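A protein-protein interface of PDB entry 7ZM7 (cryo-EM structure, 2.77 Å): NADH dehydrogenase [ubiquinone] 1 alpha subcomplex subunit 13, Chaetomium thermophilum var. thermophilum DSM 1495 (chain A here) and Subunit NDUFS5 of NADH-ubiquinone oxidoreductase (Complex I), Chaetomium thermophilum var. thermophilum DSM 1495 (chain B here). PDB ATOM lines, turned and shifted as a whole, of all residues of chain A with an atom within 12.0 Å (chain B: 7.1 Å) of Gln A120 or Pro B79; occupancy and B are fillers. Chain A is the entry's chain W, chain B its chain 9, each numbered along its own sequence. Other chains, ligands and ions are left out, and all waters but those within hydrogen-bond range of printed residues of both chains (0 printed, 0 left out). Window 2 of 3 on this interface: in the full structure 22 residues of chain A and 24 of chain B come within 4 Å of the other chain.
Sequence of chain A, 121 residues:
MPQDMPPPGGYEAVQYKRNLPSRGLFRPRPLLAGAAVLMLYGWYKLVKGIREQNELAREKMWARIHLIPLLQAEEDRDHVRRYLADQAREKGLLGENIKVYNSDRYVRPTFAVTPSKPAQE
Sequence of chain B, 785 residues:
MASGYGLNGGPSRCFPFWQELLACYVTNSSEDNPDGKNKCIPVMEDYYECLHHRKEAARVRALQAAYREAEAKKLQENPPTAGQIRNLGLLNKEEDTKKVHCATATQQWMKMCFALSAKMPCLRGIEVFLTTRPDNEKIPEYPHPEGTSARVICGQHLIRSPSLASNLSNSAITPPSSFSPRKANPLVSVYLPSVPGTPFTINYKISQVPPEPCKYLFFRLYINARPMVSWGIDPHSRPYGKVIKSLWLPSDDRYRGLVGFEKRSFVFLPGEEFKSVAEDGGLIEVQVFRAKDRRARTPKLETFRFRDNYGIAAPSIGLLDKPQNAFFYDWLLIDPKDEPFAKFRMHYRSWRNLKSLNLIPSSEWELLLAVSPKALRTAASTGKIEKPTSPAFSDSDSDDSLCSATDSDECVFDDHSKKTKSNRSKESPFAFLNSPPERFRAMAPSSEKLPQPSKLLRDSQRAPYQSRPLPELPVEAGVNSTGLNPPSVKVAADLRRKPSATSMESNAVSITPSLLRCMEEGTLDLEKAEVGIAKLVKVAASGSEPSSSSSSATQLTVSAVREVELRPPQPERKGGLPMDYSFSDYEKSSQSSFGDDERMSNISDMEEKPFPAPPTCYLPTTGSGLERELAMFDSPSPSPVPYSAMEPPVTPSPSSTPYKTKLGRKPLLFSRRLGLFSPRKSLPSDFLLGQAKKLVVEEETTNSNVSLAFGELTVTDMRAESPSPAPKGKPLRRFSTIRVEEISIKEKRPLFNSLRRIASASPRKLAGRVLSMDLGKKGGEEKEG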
ATOM      1  N   PRO A 115     -32.476 -18.194  -0.268  1.00  0.00           N
ATOM      2  CA  PRO A 115     -31.456 -18.272   0.775  1.00  0.00           C
ATOM      3  C   PRO A 115     -32.086 -18.315   2.153  1.00  0.00           C
ATOM      4  O   PRO A 115     -33.220 -17.890   2.372  1.00  0.00           O
ATOM      5  CB  PRO A 115     -30.641 -16.997   0.586  1.00  0.00           C
ATOM      6  CG  PRO A 115     -31.021 -16.473  -0.731  1.00  0.00           C
ATOM      7  CD  PRO A 115     -32.343 -16.991  -1.093  1.00  0.00           C
ATOM      8  N   SER A 116     -31.331 -18.865   3.090  1.00  0.00           N
ATOM      9  CA  SER A 116     -31.787 -18.886   4.467  1.00  0.00           C
ATOM     10  C   SER A 116     -31.709 -17.509   5.116  1.00  0.00           C
ATOM     11  O   SER A 116     -32.342 -17.287   6.150  1.00  0.00           O
ATOM     12  CB  SER A 116     -30.987 -19.925   5.244  1.00  0.00           C
ATOM     13  OG  SER A 116     -29.611 -19.822   4.938  1.00  0.00           O
ATOM     14  N   LYS A 117     -30.966 -16.570   4.532  1.00  0.00           N
ATOM     15  CA  LYS A 117     -30.866 -15.234   5.099  1.00  0.00           C
ATOM     16  C   LYS A 117     -30.949 -14.155   4.030  1.00  0.00           C
ATOM     17  O   LYS A 117     -30.514 -14.356   2.895  1.00  0.00           O
ATOM     18  CB  LYS A 117     -29.553 -15.062   5.874  1.00  0.00           C
ATOM     19  CG  LYS A 117     -29.438 -15.935   7.116  1.00  0.00           C
ATOM     20  CD  LYS A 117     -30.479 -15.553   8.152  1.00  0.00           C
ATOM     21  CE  LYS A 117     -30.110 -14.261   8.855  1.00  0.00           C
ATOM     22  NZ  LYS A 117     -28.891 -14.422   9.694  1.00  0.00           N
ATOM     23  N   PRO A 118     -31.488 -12.993   4.374  1.00  0.00           N
ATOM     24  CA  PRO A 118     -31.437 -11.853   3.454  1.00  0.00           C
ATOM     25  C   PRO A 118     -30.088 -11.162   3.457  1.00  0.00           C
ATOM     26  O   PRO A 118     -29.160 -11.594   4.145  1.00  0.00           O
ATOM     27  CB  PRO A 118     -32.524 -10.920   3.994  1.00  0.00           C
ATOM     28  CG  PRO A 118     -33.307 -11.728   4.946  1.00  0.00           C
ATOM     29  CD  PRO A 118     -32.361 -12.716   5.518  1.00  0.00           C
ATOM     30  N   ALA A 119     -29.966 -10.084   2.692  1.00  0.00           N
ATOM     31  CA  ALA A 119     -28.777  -9.255   2.765  1.00  0.00           C
ATOM     32  C   ALA A 119     -28.666  -8.614   4.143  1.00  0.00           C
ATOM     33  O   ALA A 119     -29.659  -8.432   4.854  1.00  0.00           O
ATOM     34  CB  ALA A 119     -28.805  -8.173   1.690  1.00  0.00           C
ATOM     35  N   GLN A 120     -27.435  -8.279   4.526  1.00  0.00           N
ATOM     36  CA  GLN A 120     -27.196  -7.733   5.858  1.00  0.00           C
ATOM     37  C   GLN A 120     -27.924  -6.409   6.052  1.00  0.00           C
ATOM     38  O   GLN A 120     -28.484  -6.147   7.121  1.00  0.00           O
ATOM     39  CB  GLN A 120     -25.696  -7.568   6.097  1.00  0.00           C
ATOM     40  CG  GLN A 120     -25.018  -8.823   6.615  1.00  0.00           C
ATOM     41  CD  GLN A 120     -25.013  -9.944   5.597  1.00  0.00           C
ATOM     42  OE1 GLN A 120     -25.547 -11.024   5.844  1.00  0.00           O
ATOM     43  NE2 GLN A 120     -24.411  -9.691   4.443  1.00  0.00           N
ATOM     44  N   GLU A 121     -27.921  -5.563   5.026  1.00  0.00           N
ATOM     45  CA  GLU A 121     -28.556  -4.247   5.082  1.00  0.00           C
ATOM     46  C   GLU A 121     -27.987  -3.403   6.217  1.00  0.00           C
ATOM     47  O   GLU A 121     -26.780  -3.406   6.458  1.00  0.00           O
ATOM     48  CB  GLU A 121     -30.073  -4.379   5.238  1.00  0.00           C
ATOM     49  N   GLN B  76     -17.249 -17.706   1.582  1.00  0.00           N
ATOM     50  CA  GLN B  76     -17.897 -16.476   1.146  1.00  0.00           C
ATOM     51  C   GLN B  76     -16.848 -15.378   1.031  1.00  0.00           C
ATOM     52  O   GLN B  76     -16.111 -15.112   1.987  1.00  0.00           O
ATOM     53  CB  GLN B  76     -19.012 -16.075   2.113  1.00  0.00           C
ATOM     54  CG  GLN B  76     -18.635 -16.148   3.584  1.00  0.00           C
ATOM     55  CD  GLN B  76     -18.111 -14.832   4.122  1.00  0.00           C
ATOM     56  OE1 GLN B  76     -18.416 -13.765   3.588  1.00  0.00           O
ATOM     57  NE2 GLN B  76     -17.320 -14.900   5.185  1.00  0.00           N
ATOM     58  N   GLU B  77     -16.769 -14.755  -0.143  1.00  0.00           N
ATOM     59  CA  GLU B  77     -15.761 -13.724  -0.365  1.00  0.00           C
ATOM     60  C   GLU B  77     -16.227 -12.372   0.162  1.00  0.00           C
ATOM     61  O   GLU B  77     -15.630 -11.811   1.086  1.00  0.00           O
ATOM     62  CB  GLU B  77     -15.426 -13.637  -1.856  1.00  0.00           C
ATOM     63  CG  GLU B  77     -15.257 -14.989  -2.529  1.00  0.00           C
ATOM     64  CD  GLU B  77     -14.083 -15.774  -1.980  1.00  0.00           C
ATOM     65  OE1 GLU B  77     -13.075 -15.146  -1.593  1.00  0.00           O
ATOM     66  OE2 GLU B  77     -14.170 -17.018  -1.934  1.00  0.00           O
ATOM     67  N   ASN B  78     -17.303 -11.843  -0.410  1.00  0.00           N
ATOM     68  CA  ASN B  78     -17.838 -10.546  -0.025  1.00  0.00           C
ATOM     69  C   ASN B  78     -19.324 -10.495  -0.349  1.00  0.00           C
ATOM     70  O   ASN B  78     -19.700 -10.248  -1.502  1.00  0.00           O
ATOM     71  CB  ASN B  78     -17.097  -9.419  -0.744  1.00  0.00           C
ATOM     72  CG  ASN B  78     -15.843  -8.989  -0.014  1.00  0.00           C
ATOM     73  OD1 ASN B  78     -15.847  -8.824   1.205  1.00  0.00           O
ATOM     74  ND2 ASN B  78     -14.761  -8.806  -0.757  1.00  0.00           N
ATOM     75  N   PRO B  79     -20.195 -10.724   0.625  1.00  0.00           N
ATOM     76  CA  PRO B  79     -21.631 -10.729   0.349  1.00  0.00           C
ATOM     77  C   PRO B  79     -22.117  -9.338  -0.010  1.00  0.00           C
ATOM     78  O   PRO B  79     -21.844  -8.367   0.712  1.00  0.00           O
ATOM     79  CB  PRO B  79     -22.242 -11.212   1.672  1.00  0.00           C
ATOM     80  CG  PRO B  79     -21.241 -10.827   2.702  1.00  0.00           C
ATOM     81  CD  PRO B  79     -19.899 -10.965   2.047  1.00  0.00           C
ATOM     82  N   PRO B  80     -22.832  -9.198  -1.122  1.00  0.00           N
ATOM     83  CA  PRO B  80     -23.335  -7.877  -1.510  1.00  0.00           C
ATOM     84  C   PRO B  80     -24.431  -7.413  -0.567  1.00  0.00           C
ATOM     85  O   PRO B  80     -25.349  -8.165  -0.237  1.00  0.00           O
ATOM     86  CB  PRO B  80     -23.876  -8.106  -2.925  1.00  0.00           C
ATOM     87  CG  PRO B  80     -23.259  -9.400  -3.375  1.00  0.00           C
ATOM     88  CD  PRO B  80     -23.129 -10.217  -2.137  1.00  0.00           C
ATOM     89  N   THR B  81     -24.327  -6.168  -0.128  1.00  0.00           N
ATOM     90  CA  THR B  81     -25.320  -5.626   0.782  1.00  0.00           C
ATOM     91  C   THR B  81     -26.603  -5.320   0.025  1.00  0.00           C
ATOM     92  O   THR B  81     -26.631  -5.287  -1.206  1.00  0.00           O
ATOM     93  CB  THR B  81     -24.804  -4.368   1.475  1.00  0.00           C
ATOM     94  OG1 THR B  81     -25.633  -4.081   2.607  1.00  0.00           O
ATOM     95  CG2 THR B  81     -24.841  -3.186   0.529  1.00  0.00           C
ATOM     96  N   ALA B  82     -27.681  -5.117   0.779  1.00  0.00           N
ATOM     97  CA  ALA B  82     -28.963  -4.856   0.141  1.00  0.00           C
ATOM     98  C   ALA B  82     -28.911  -3.571  -0.667  1.00  0.00           C
ATOM     99  O   ALA B  82     -29.433  -3.511  -1.786  1.00  0.00           O
ATOM    100  CB  ALA B  82     -30.079  -4.797   1.184  1.00  0.00           C
ATOM    101  N   GLN B  84     -26.482  -2.342  -2.259  1.00  0.00           N
ATOM    102  CA  GLN B  84     -25.830  -2.614  -3.533  1.00  0.00           C
ATOM    103  C   GLN B  84     -26.775  -3.303  -4.506  1.00  0.00           C
ATOM    104  O   GLN B  84     -26.855  -2.915  -5.674  1.00  0.00           O
ATOM    105  CB  GLN B  84     -24.576  -3.448  -3.303  1.00  0.00           C
ATOM    106  CG  GLN B  84     -23.446  -2.667  -2.682  1.00  0.00           C
ATOM    107  CD  GLN B  84     -22.280  -3.544  -2.284  1.00  0.00           C
ATOM    108  OE1 GLN B  84     -22.447  -4.522  -1.557  1.00  0.00           O
ATOM    109  NE2 GLN B  84     -21.088  -3.190  -2.744  1.00  0.00           N
ATOM    110  N   LYS B  99     -20.128  -5.475  -9.118  1.00  0.00           N
ATOM    111  CA  LYS B  99     -19.911  -6.241  -7.898  1.00  0.00           C
ATOM    112  C   LYS B  99     -20.963  -7.328  -7.734  1.00  0.00           C
ATOM    113  O   LYS B  99     -20.649  -8.441  -7.298  1.00  0.00           O
ATOM    114  CB  LYS B  99     -19.904  -5.313  -6.688  1.00  0.00           C
ATOM    115  CG  LYS B  99     -19.678  -6.029  -5.373  1.00  0.00           C
ATOM    116  CD  LYS B  99     -18.378  -6.810  -5.401  1.00  0.00           C
ATOM    117  CE  LYS B  99     -17.174  -5.889  -5.487  1.00  0.00           C
ATOM    118  NZ  LYS B  99     -15.901  -6.659  -5.517  1.00  0.00           N
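The side-chain amide oxygen (OE1) of Gln B84 is in hydrogen-bond range of the backbone NH (N) of Thr B81.
Among the printed residues, pairs that only touch across the chains: Ala A119 with Ala B82 (3.4 Å), Glu A121 with Thr B81 (3.6 Å), Gln A120 with Pro B79 (3.8 Å), Ala A119 with Pro B80 (3.96 Å) and Ala A119 with Thr B81 (3.97 Å).
Of the printed residues of chain B, Ala A119 touches Pro B80, Thr B81 and Ala B82.
Of chain B, only Pro B79 (3.8 Å) comes within 4 Å of Gln A120.
Of the printed residues of chain B, Glu A121 touches Thr B81.
No residue of chain A comes within 4 Å of Gln B76.
Pro B79 touches just one residue of chain A: Gln A120 (3.8 Å).
Of the printed residues of chain A, Ala B82 touches Ala A119 (3.4 Å).
The nearest residue of chain B that does not touch Gln A120 is Thr B81 (4.7 Å).
The nearest residue of chain A that does not touch Pro B79 is Ala A119 (6.9 Å).
The nearest printed residue of chain A that does not touch Ala B82 is Glu A121 (4.1 Å).
Of the 7 printed residues of chain A, 3 touch a printed residue of chain B.
Hydrophobic or aromatic side chains of chain A that line the printed part of chain B: Ala A119.
Among the printed residues, no Asp or Glu carboxylate lies within 4 Å of a Lys or Arg side-chain nitrogen of the other chain.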
